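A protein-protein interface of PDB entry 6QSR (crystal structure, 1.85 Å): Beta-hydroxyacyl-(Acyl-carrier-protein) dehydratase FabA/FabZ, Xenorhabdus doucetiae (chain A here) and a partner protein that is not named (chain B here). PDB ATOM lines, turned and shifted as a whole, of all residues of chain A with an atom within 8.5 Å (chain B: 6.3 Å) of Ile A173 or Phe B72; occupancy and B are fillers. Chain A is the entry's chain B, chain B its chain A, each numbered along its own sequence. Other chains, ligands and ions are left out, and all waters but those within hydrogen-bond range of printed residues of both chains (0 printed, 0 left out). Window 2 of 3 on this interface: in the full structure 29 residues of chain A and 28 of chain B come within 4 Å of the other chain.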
ATOM      1  N   LEU A 105      21.700   0.677  -5.587  1.00  0.00           N
ATOM      2  CA  LEU A 105      22.513  -0.474  -5.204  1.00  0.00           C
ATOM      3  C   LEU A 105      22.800  -1.337  -6.408  1.00  0.00           C
ATOM      4  O   LEU A 105      21.947  -1.497  -7.272  1.00  0.00           O
ATOM      5  CB  LEU A 105      21.765  -1.340  -4.192  1.00  0.00           C
ATOM      6  CG  LEU A 105      21.561  -0.784  -2.787  1.00  0.00           C
ATOM      7  CD1 LEU A 105      20.425  -1.529  -2.106  1.00  0.00           C
ATOM      8  CD2 LEU A 105      22.846  -0.864  -1.980  1.00  0.00           C
ATOM      9  N   MET A 107      24.974  -5.196  -7.321  1.00  0.00           N
ATOM     10  CA  MET A 107      25.679  -6.344  -6.787  1.00  0.00           C
ATOM     11  C   MET A 107      26.180  -7.219  -7.906  1.00  0.00           C
ATOM     12  O   MET A 107      25.459  -7.484  -8.867  1.00  0.00           O
ATOM     13  CB  MET A 107      24.750  -7.190  -5.933  1.00  0.00           C
ATOM     14  CG  MET A 107      24.203  -6.490  -4.714  1.00  0.00           C
ATOM     15  SD  MET A 107      23.206  -7.683  -3.822  1.00  0.00           S
ATOM     16  CE  MET A 107      23.828  -7.399  -2.178  1.00  0.00           C
ATOM     17  N   LEU A 108      27.412  -7.679  -7.751  1.00  0.00           N
ATOM     18  CA  LEU A 108      27.937  -8.727  -8.584  1.00  0.00           C
ATOM     19  C   LEU A 108      27.602 -10.050  -7.889  1.00  0.00           C
ATOM     20  O   LEU A 108      27.935 -10.238  -6.712  1.00  0.00           O
ATOM     21  CB  LEU A 108      29.438  -8.528  -8.752  1.00  0.00           C
ATOM     22  CG  LEU A 108      30.154  -9.413  -9.766  1.00  0.00           C
ATOM     23  CD1 LEU A 108      29.657  -9.176 -11.179  1.00  0.00           C
ATOM     24  CD2 LEU A 108      31.644  -9.148  -9.662  1.00  0.00           C
ATOM     25  N   LEU A 109      26.896 -10.934  -8.600  1.00  0.00           N
ATOM     26  CA  LEU A 109      26.532 -12.268  -8.093  1.00  0.00           C
ATOM     27  C   LEU A 109      27.546 -13.339  -8.491  1.00  0.00           C
ATOM     28  O   LEU A 109      27.689 -14.352  -7.806  1.00  0.00           O
ATOM     29  CB  LEU A 109      25.177 -12.711  -8.649  1.00  0.00           C
ATOM     30  CG  LEU A 109      23.901 -11.933  -8.334  1.00  0.00           C
ATOM     31  CD1 LEU A 109      22.710 -12.659  -8.958  1.00  0.00           C
ATOM     32  CD2 LEU A 109      23.724 -11.766  -6.831  1.00  0.00           C
ATOM     33  N   ASN A 165      16.374  -3.601  -4.486  1.00  0.00           N
ATOM     34  CA  ASN A 165      15.908  -2.490  -3.654  1.00  0.00           C
ATOM     35  C   ASN A 165      16.617  -2.569  -2.312  1.00  0.00           C
ATOM     36  O   ASN A 165      17.064  -3.644  -1.908  1.00  0.00           O
ATOM     37  CB  ASN A 165      14.396  -2.574  -3.392  1.00  0.00           C
ATOM     38  CG  ASN A 165      13.565  -2.272  -4.620  1.00  0.00           C
ATOM     39  OD1 ASN A 165      13.844  -2.767  -5.711  1.00  0.00           O
ATOM     40  ND2 ASN A 165      12.525  -1.464  -4.446  1.00  0.00           N
ATOM     41  N   LYS A 166      16.685  -1.436  -1.617  1.00  0.00           N
ATOM     42  CA  LYS A 166      17.196  -1.385  -0.241  1.00  0.00           C
ATOM     43  C   LYS A 166      16.424  -2.322   0.705  1.00  0.00           C
ATOM     44  O   LYS A 166      17.031  -2.967   1.560  1.00  0.00           O
ATOM     45  CB  LYS A 166      17.158   0.058   0.277  1.00  0.00           C
ATOM     46  CG  LYS A 166      17.504   0.256   1.745  1.00  0.00           C
ATOM     47  CD  LYS A 166      18.918  -0.179   2.084  1.00  0.00           C
ATOM     48  CE  LYS A 166      19.255   0.253   3.503  1.00  0.00           C
ATOM     49  NZ  LYS A 166      20.639  -0.107   3.900  1.00  0.00           N
ATOM     50  N   THR A 167      15.100  -2.394   0.549  1.00  0.00           N
ATOM     51  CA  THR A 167      14.255  -3.264   1.384  1.00  0.00           C
ATOM     52  C   THR A 167      14.501  -4.740   1.090  1.00  0.00           C
ATOM     53  O   THR A 167      14.527  -5.568   2.002  1.00  0.00           O
ATOM     54  CB  THR A 167      12.758  -2.946   1.190  1.00  0.00           C
ATOM     55  OG1 THR A 167      12.538  -1.548   1.408  1.00  0.00           O
ATOM     56  CG2 THR A 167      11.889  -3.748   2.163  1.00  0.00           C
ATOM     57  N   GLU A 168      14.682  -5.057  -0.189  1.00  0.00           N
ATOM     58  CA  GLU A 168      15.029  -6.410  -0.624  1.00  0.00           C
ATOM     59  C   GLU A 168      16.347  -6.855   0.020  1.00  0.00           C
ATOM     60  O   GLU A 168      16.471  -7.983   0.505  1.00  0.00           O
ATOM     61  CB  GLU A 168      15.135  -6.432  -2.151  1.00  0.00           C
ATOM     62  CG  GLU A 168      15.144  -7.808  -2.787  1.00  0.00           C
ATOM     63  CD  GLU A 168      15.093  -7.748  -4.309  1.00  0.00           C
ATOM     64  OE1 GLU A 168      15.101  -8.827  -4.938  1.00  0.00           O
ATOM     65  OE2 GLU A 168      15.054  -6.630  -4.879  1.00  0.00           O
ATOM     66  N   LEU A 169      17.311  -5.943   0.040  1.00  0.00           N
ATOM     67  CA  LEU A 169      18.609  -6.183   0.662  1.00  0.00           C
ATOM     68  C   LEU A 169      18.521  -6.415   2.175  1.00  0.00           C
ATOM     69  O   LEU A 169      19.204  -7.296   2.701  1.00  0.00           O
ATOM     70  CB  LEU A 169      19.547  -5.014   0.354  1.00  0.00           C
ATOM     71  CG  LEU A 169      21.014  -5.163   0.731  1.00  0.00           C
ATOM     72  CD1 LEU A 169      21.644  -6.340   0.013  1.00  0.00           C
ATOM     73  CD2 LEU A 169      21.737  -3.874   0.380  1.00  0.00           C
ATOM     74  N   ILE A 170      17.686  -5.631   2.861  1.00  0.00           N
ATOM     75  CA  ILE A 170      17.410  -5.825   4.299  1.00  0.00           C
ATOM     76  C   ILE A 170      16.817  -7.210   4.571  1.00  0.00           C
ATOM     77  O   ILE A 170      17.232  -7.892   5.512  1.00  0.00           O
ATOM     78  CB  ILE A 170      16.451  -4.734   4.859  1.00  0.00           C
ATOM     79  CG1 ILE A 170      17.155  -3.372   4.910  1.00  0.00           C
ATOM     80  CG2 ILE A 170      15.941  -5.103   6.255  1.00  0.00           C
ATOM     81  CD1 ILE A 170      16.218  -2.175   4.899  1.00  0.00           C
ATOM     82  N   GLN A 171      15.827  -7.591   3.765  1.00  0.00           N
ATOM     83  CA  GLN A 171      15.212  -8.924   3.841  1.00  0.00           C
ATOM     84  C   GLN A 171      16.228 -10.040   3.587  1.00  0.00           C
ATOM     85  O   GLN A 171      16.208 -11.064   4.269  1.00  0.00           O
ATOM     86  CB  GLN A 171      14.032  -9.036   2.863  1.00  0.00           C
ATOM     87  CG  GLN A 171      12.821  -8.206   3.284  1.00  0.00           C
ATOM     88  CD  GLN A 171      11.747  -8.091   2.213  1.00  0.00           C
ATOM     89  OE1 GLN A 171      10.995  -7.117   2.182  1.00  0.00           O
ATOM     90  NE2 GLN A 171      11.660  -9.086   1.340  1.00  0.00           N
ATOM     91  N   LEU A 172      17.121  -9.820   2.619  1.00  0.00           N
ATOM     92  CA  LEU A 172      18.214 -10.759   2.317  1.00  0.00           C
ATOM     93  C   LEU A 172      19.148 -10.899   3.526  1.00  0.00           C
ATOM     94  O   LEU A 172      19.431 -12.014   3.970  1.00  0.00           O
ATOM     95  CB  LEU A 172      19.006 -10.285   1.084  1.00  0.00           C
ATOM     96  CG  LEU A 172      19.729 -11.302   0.191  1.00  0.00           C
ATOM     97  CD1 LEU A 172      20.503 -10.548  -0.881  1.00  0.00           C
ATOM     98  CD2 LEU A 172      20.659 -12.232   0.954  1.00  0.00           C
ATOM     99  N   ILE A 173      19.604  -9.760   4.052  1.00  0.00           N
ATOM    100  CA  ILE A 173      20.493  -9.719   5.222  1.00  0.00           C
ATOM    101  C   ILE A 173      19.880 -10.405   6.455  1.00  0.00           C
ATOM    102  O   ILE A 173      20.602 -11.052   7.217  1.00  0.00           O
ATOM    103  CB  ILE A 173      20.912  -8.259   5.563  1.00  0.00           C
ATOM    104  CG1 ILE A 173      21.863  -7.719   4.486  1.00  0.00           C
ATOM    105  CG2 ILE A 173      21.594  -8.163   6.930  1.00  0.00           C
ATOM    106  CD1 ILE A 173      21.915  -6.208   4.401  1.00  0.00           C
ATOM    107  N   ASN A 174      18.562 -10.275   6.635  1.00  0.00           N
ATOM    108  CA  ASN A 174      17.885 -10.714   7.862  1.00  0.00           C
ATOM    109  C   ASN A 174      17.127 -12.048   7.784  1.00  0.00           C
ATOM    110  O   ASN A 174      16.961 -12.699   8.817  1.00  0.00           O
ATOM    111  CB  ASN A 174      16.933  -9.611   8.349  1.00  0.00           C
ATOM    112  CG  ASN A 174      17.670  -8.456   8.996  1.00  0.00           C
ATOM    113  OD1 ASN A 174      17.774  -7.369   8.430  1.00  0.00           O
ATOM    114  ND2 ASN A 174      18.205  -8.694  10.183  1.00  0.00           N
ATOM    115  N   LYS A 175      16.662 -12.449   6.597  1.00  0.00           N
ATOM    116  CA  LYS A 175      15.851 -13.673   6.455  1.00  0.00           C
ATOM    117  C   LYS A 175      16.668 -14.803   5.847  1.00  0.00           C
ATOM    118  O   LYS A 175      17.116 -15.700   6.561  1.00  0.00           O
ATOM    119  CB  LYS A 175      14.590 -13.411   5.619  1.00  0.00           C
ATOM    120  CG  LYS A 175      13.589 -12.473   6.293  1.00  0.00           C
ATOM    121  CD  LYS A 175      12.767 -11.648   5.305  1.00  0.00           C
ATOM    122  CE  LYS A 175      11.488 -12.339   4.849  1.00  0.00           C
ATOM    123  NZ  LYS A 175      11.679 -13.743   4.383  1.00  0.00           N
ATOM    124  N   GLN B  36      23.710   1.974   1.478  1.00  0.00           N
ATOM    125  CA  GLN B  36      24.180   0.795   2.214  1.00  0.00           C
ATOM    126  C   GLN B  36      25.649   0.555   1.896  1.00  0.00           C
ATOM    127  O   GLN B  36      25.972   0.337   0.718  1.00  0.00           O
ATOM    128  CB  GLN B  36      23.404  -0.458   1.790  1.00  0.00           C
ATOM    129  CG  GLN B  36      23.973  -1.778   2.327  1.00  0.00           C
ATOM    130  CD  GLN B  36      23.771  -1.960   3.817  1.00  0.00           C
ATOM    131  OE1 GLN B  36      22.673  -1.757   4.327  1.00  0.00           O
ATOM    132  NE2 GLN B  36      24.825  -2.371   4.519  1.00  0.00           N
ATOM    133  N   LEU B  38      28.432  -1.811   1.199  1.00  0.00           N
ATOM    134  CA  LEU B  38      28.577  -3.223   0.853  1.00  0.00           C
ATOM    135  C   LEU B  38      29.993  -3.455   0.384  1.00  0.00           C
ATOM    136  O   LEU B  38      30.537  -2.631  -0.352  1.00  0.00           O
ATOM    137  CB  LEU B  38      27.632  -3.609  -0.284  1.00  0.00           C
ATOM    138  CG  LEU B  38      26.140  -3.641   0.020  1.00  0.00           C
ATOM    139  CD1 LEU B  38      25.368  -3.849  -1.274  1.00  0.00           C
ATOM    140  CD2 LEU B  38      25.821  -4.735   1.031  1.00  0.00           C
ATOM    141  N   GLN B  44      37.074  -8.866  -2.175  1.00  0.00           N
ATOM    142  CA  GLN B  44      37.179 -10.245  -1.696  1.00  0.00           C
ATOM    143  C   GLN B  44      38.209 -11.038  -2.513  1.00  0.00           C
ATOM    144  O   GLN B  44      38.977 -11.826  -1.954  1.00  0.00           O
ATOM    145  CB  GLN B  44      35.807 -10.934  -1.726  1.00  0.00           C
ATOM    146  CG  GLN B  44      34.770 -10.288  -0.800  1.00  0.00           C
ATOM    147  CD  GLN B  44      33.380 -10.880  -0.975  1.00  0.00           C
ATOM    148  OE1 GLN B  44      33.197 -12.091  -0.886  1.00  0.00           O
ATOM    149  NE2 GLN B  44      32.391 -10.022  -1.225  1.00  0.00           N
ATOM    150  N   PHE B  70      29.192 -14.929  -5.379  1.00  0.00           N
ATOM    151  CA  PHE B  70      28.956 -14.073  -4.232  1.00  0.00           C
ATOM    152  C   PHE B  70      27.509 -14.302  -3.848  1.00  0.00           C
ATOM    153  O   PHE B  70      26.593 -13.844  -4.539  1.00  0.00           O
ATOM    154  CB  PHE B  70      29.207 -12.616  -4.602  1.00  0.00           C
ATOM    155  CG  PHE B  70      30.595 -12.353  -5.103  1.00  0.00           C
ATOM    156  CD1 PHE B  70      30.846 -12.179  -6.465  1.00  0.00           C
ATOM    157  CD2 PHE B  70      31.659 -12.302  -4.214  1.00  0.00           C
ATOM    158  CE1 PHE B  70      32.130 -11.931  -6.916  1.00  0.00           C
ATOM    159  CE2 PHE B  70      32.947 -12.063  -4.660  1.00  0.00           C
ATOM    160  CZ  PHE B  70      33.183 -11.875  -6.018  1.00  0.00           C
ATOM    161  N   GLN B  71      27.302 -15.023  -2.753  1.00  0.00           N
ATOM    162  CA  GLN B  71      25.969 -15.512  -2.397  1.00  0.00           C
ATOM    163  C   GLN B  71      25.347 -14.873  -1.151  1.00  0.00           C
ATOM    164  O   GLN B  71      24.217 -15.213  -0.809  1.00  0.00           O
ATOM    165  CB  GLN B  71      25.987 -17.043  -2.286  1.00  0.00           C
ATOM    166  CG  GLN B  71      26.697 -17.620  -1.073  1.00  0.00           C
ATOM    167  CD  GLN B  71      27.132 -19.063  -1.282  1.00  0.00           C
ATOM    168  OE1 GLN B  71      28.111 -19.335  -1.981  1.00  0.00           O
ATOM    169  NE2 GLN B  71      26.409 -19.996  -0.672  1.00  0.00           N
ATOM    170  N   PHE B  72      26.060 -13.953  -0.492  1.00  0.00           N
ATOM    171  CA  PHE B  72      25.514 -13.200   0.649  1.00  0.00           C
ATOM    172  C   PHE B  72      26.215 -11.841   0.757  1.00  0.00           C
ATOM    173  O   PHE B  72      27.443 -11.793   0.668  1.00  0.00           O
ATOM    174  CB  PHE B  72      25.709 -13.995   1.948  1.00  0.00           C
ATOM    175  CG  PHE B  72      24.832 -13.538   3.084  1.00  0.00           C
ATOM    176  CD1 PHE B  72      25.306 -12.637   4.036  1.00  0.00           C
ATOM    177  CD2 PHE B  72      23.526 -14.012   3.206  1.00  0.00           C
ATOM    178  CE1 PHE B  72      24.493 -12.217   5.091  1.00  0.00           C
ATOM    179  CE2 PHE B  72      22.713 -13.596   4.259  1.00  0.00           C
ATOM    180  CZ  PHE B  72      23.198 -12.695   5.200  1.00  0.00           C
ATOM    181  N   PRO B  73      25.452 -10.738   0.957  1.00  0.00           N
ATOM    182  CA  PRO B  73      26.114  -9.430   1.046  1.00  0.00           C
ATOM    183  C   PRO B  73      26.882  -9.235   2.349  1.00  0.00           C
ATOM    184  O   PRO B  73      26.434  -9.687   3.413  1.00  0.00           O
ATOM    185  CB  PRO B  73      24.964  -8.423   0.957  1.00  0.00           C
ATOM    186  CG  PRO B  73      23.725  -9.175   1.304  1.00  0.00           C
ATOM    187  CD  PRO B  73      24.002 -10.647   1.233  1.00  0.00           C
ATOM    188  N   LEU B  74      28.029  -8.568   2.249  1.00  0.00           N
ATOM    189  CA  LEU B  74      28.888  -8.289   3.389  1.00  0.00           C
ATOM    190  C   LEU B  74      28.936  -6.791   3.632  1.00  0.00           C
ATOM    191  O   LEU B  74      28.985  -6.005   2.689  1.00  0.00           O
ATOM    192  CB  LEU B  74      30.294  -8.832   3.130  1.00  0.00           C
ATOM    193  CG  LEU B  74      30.355 -10.357   2.949  1.00  0.00           C
ATOM    194  CD1 LEU B  74      31.757 -10.802   2.585  1.00  0.00           C
ATOM    195  CD2 LEU B  74      29.894 -11.069   4.212  1.00  0.00           C
ATOM    196  N   GLN B  75      28.910  -6.410   4.905  1.00  0.00           N
ATOM    197  CA  GLN B  75      28.834  -5.006   5.317  1.00  0.00           C
ATOM    198  C   GLN B  75      29.749  -4.747   6.515  1.00  0.00           C
ATOM    199  O   GLN B  75      30.239  -5.695   7.136  1.00  0.00           O
ATOM    200  CB  GLN B  75      27.381  -4.633   5.652  1.00  0.00           C
ATOM    201  CG  GLN B  75      26.769  -5.375   6.828  1.00  0.00           C
ATOM    202  CD  GLN B  75      25.384  -4.860   7.188  1.00  0.00           C
ATOM    203  OE1 GLN B  75      25.065  -3.686   6.986  1.00  0.00           O
ATOM    204  NE2 GLN B  75      24.557  -5.740   7.735  1.00  0.00           N
ATOM    205  N   ASN B  78      30.860  -6.962  10.054  1.00  0.00           N
ATOM    206  CA  ASN B  78      30.969  -8.404   9.833  1.00  0.00           C
ATOM    207  C   ASN B  78      32.384  -8.897  10.112  1.00  0.00           C
ATOM    208  O   ASN B  78      33.370  -8.195   9.861  1.00  0.00           O
ATOM    209  CB  ASN B  78      30.596  -8.799   8.400  1.00  0.00           C
ATOM    210  CG  ASN B  78      29.120  -8.604   8.074  1.00  0.00           C
ATOM    211  OD1 ASN B  78      28.751  -8.597   6.902  1.00  0.00           O
ATOM    212  ND2 ASN B  78      28.274  -8.459   9.092  1.00  0.00           N
ATOM    213  N   LEU B  99      30.748 -16.238   6.868  1.00  0.00           N
ATOM    214  CA  LEU B  99      30.380 -15.338   7.961  1.00  0.00           C
ATOM    215  C   LEU B  99      30.679 -16.048   9.278  1.00  0.00           C
ATOM    216  O   LEU B  99      30.313 -17.215   9.455  1.00  0.00           O
ATOM    217  CB  LEU B  99      28.909 -14.916   7.876  1.00  0.00           C
ATOM    218  CG  LEU B  99      28.646 -13.582   7.171  1.00  0.00           C
ATOM    219  CD1 LEU B  99      27.163 -13.434   6.868  1.00  0.00           C
ATOM    220  CD2 LEU B  99      29.122 -12.408   8.020  1.00  0.00           C
ATOM    221  N   GLN B 108      25.750 -18.071   6.038  1.00  0.00           N
ATOM    222  CA  GLN B 108      26.977 -18.768   6.406  1.00  0.00           C
ATOM    223  C   GLN B 108      28.075 -18.512   5.359  1.00  0.00           C
ATOM    224  O   GLN B 108      28.924 -17.659   5.595  1.00  0.00           O
ATOM    225  CB  GLN B 108      26.698 -20.264   6.642  1.00  0.00           C
ATOM    226  CG  GLN B 108      27.915 -21.164   6.862  1.00  0.00           C
ATOM    227  CD  GLN B 108      28.825 -20.732   8.007  1.00  0.00           C
ATOM    228  OE1 GLN B 108      30.023 -21.022   7.990  1.00  0.00           O
ATOM    229  NE2 GLN B 108      28.266 -20.052   9.007  1.00  0.00           N
ATOM    230  N   THR B 109      28.062 -19.214   4.220  1.00  0.00           N
ATOM    231  CA  THR B 109      29.040 -18.952   3.148  1.00  0.00           C
ATOM    232  C   THR B 109      28.643 -17.679   2.407  1.00  0.00           C
ATOM    233  O   THR B 109      27.514 -17.557   1.938  1.00  0.00           O
ATOM    234  CB  THR B 109      29.164 -20.112   2.140  1.00  0.00           C
ATOM    235  OG1 THR B 109      29.539 -21.307   2.825  1.00  0.00           O
ATOM    236  CG2 THR B 109      30.235 -19.807   1.076  1.00  0.00           C
ATOM    237  N   ALA B 110      29.570 -16.731   2.341  1.00  0.00           N
ATOM    238  CA  ALA B 110      29.341 -15.458   1.689  1.00  0.00           C
ATOM    239  C   ALA B 110      29.793 -15.547   0.241  1.00  0.00           C
ATOM    240  O   ALA B 110      29.091 -15.097  -0.663  1.00  0.00           O
ATOM    241  CB  ALA B 110      30.080 -14.347   2.415  1.00  0.00           C
ATOM    242  N   SER B 111      30.968 -16.122   0.017  1.00  0.00           N
ATOM    243  CA  SER B 111      31.466 -16.279  -1.347  1.00  0.00           C
ATOM    244  C   SER B 111      32.423 -17.451  -1.481  1.00  0.00           C
ATOM    245  O   SER B 111      32.965 -17.949  -0.503  1.00  0.00           O
ATOM    246  CB  SER B 111      32.134 -14.984  -1.815  1.00  0.00           C
ATOM    247  OG  SER B 111      33.312 -14.729  -1.081  1.00  0.00           O
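Of the 15 printed residues of chain B, 6 touch a printed residue of chain A. Hydrophobic or aromatic side chains of chain B that line the printed part of chain A: Leu B38, Phe B70, Phe B72 and Pro B73. Among the printed residues, 15 pairs touch across the chains. Among the printed residues, no Asp or Glu carboxylate lies within 4 Å of a Lys or Arg side-chain nitrogen of the other chain.
The side-chain amide nitrogen (NE2) of Gln B36 sits at hydrogen-bond distance from the side-chain amide oxygen (OE1) of Gln B75, 2.8 Å away. O of Ala B110 is in hydrogen-bond range of N of Phe B72 (3.2 Å). The backbone NH of Gln B75 is in hydrogen-bond range of the side-chain amide oxygen of Asn B78 (3.0 Å).
Leu A105 touches Gln B36. Leu A105 touches Leu B38 (CD2 to CD1, 3.97 Å). Leu B38 touches Met A107 (CD1 to CE, 3.97 Å). Pro B73 touches Met A107 (CB to CE, 3.5 Å). CG of Gln B36 touches CD2 of Leu A169 (3.6 Å). Leu A169 touches Leu B38 (CD2 to CD1, 3.99 Å). CD1 of Leu A169 touches CG of Pro B73, 3.7 Å away. Leu A172 touches Phe B72 (O to CE2, 3.7 Å). Leu A172 touches Pro B73. Pro B73 touches Ile A173 (CG to CG1, 3.96 Å).
Of the printed residues of chain B, Met A107 touches Leu B38 (3.97 Å) and Pro B73 (3.5 Å). Of the printed residues of chain B, Leu A108 touches Phe B70. Printed residues of chain B within 4 Å of Lys A166: Gln B36 (2.7 Å). Gln A171 touches none of the printed residues of chain B. Of chain B, only Phe B72, Pro B73 and Gln B75 come within 4 Å of Ile A173. Phe B72 touches just these residues of chain A: Leu A172 and Ile A173. Pro B73 touches four residues of chain A. Ser B111 touches none of the printed residues of chain A. The nearest printed residue of chain B that does not touch Lys A166 is Gln B75 (6.5 Å).
The side-chain amino group of Lys A166 is in hydrogen-bond range of the side-chain amide oxygen of Gln B36. The backbone NH (N) of Phe B70 lies within hydrogen-bond range of the backbone carbonyl oxygen (O) of Leu A109.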
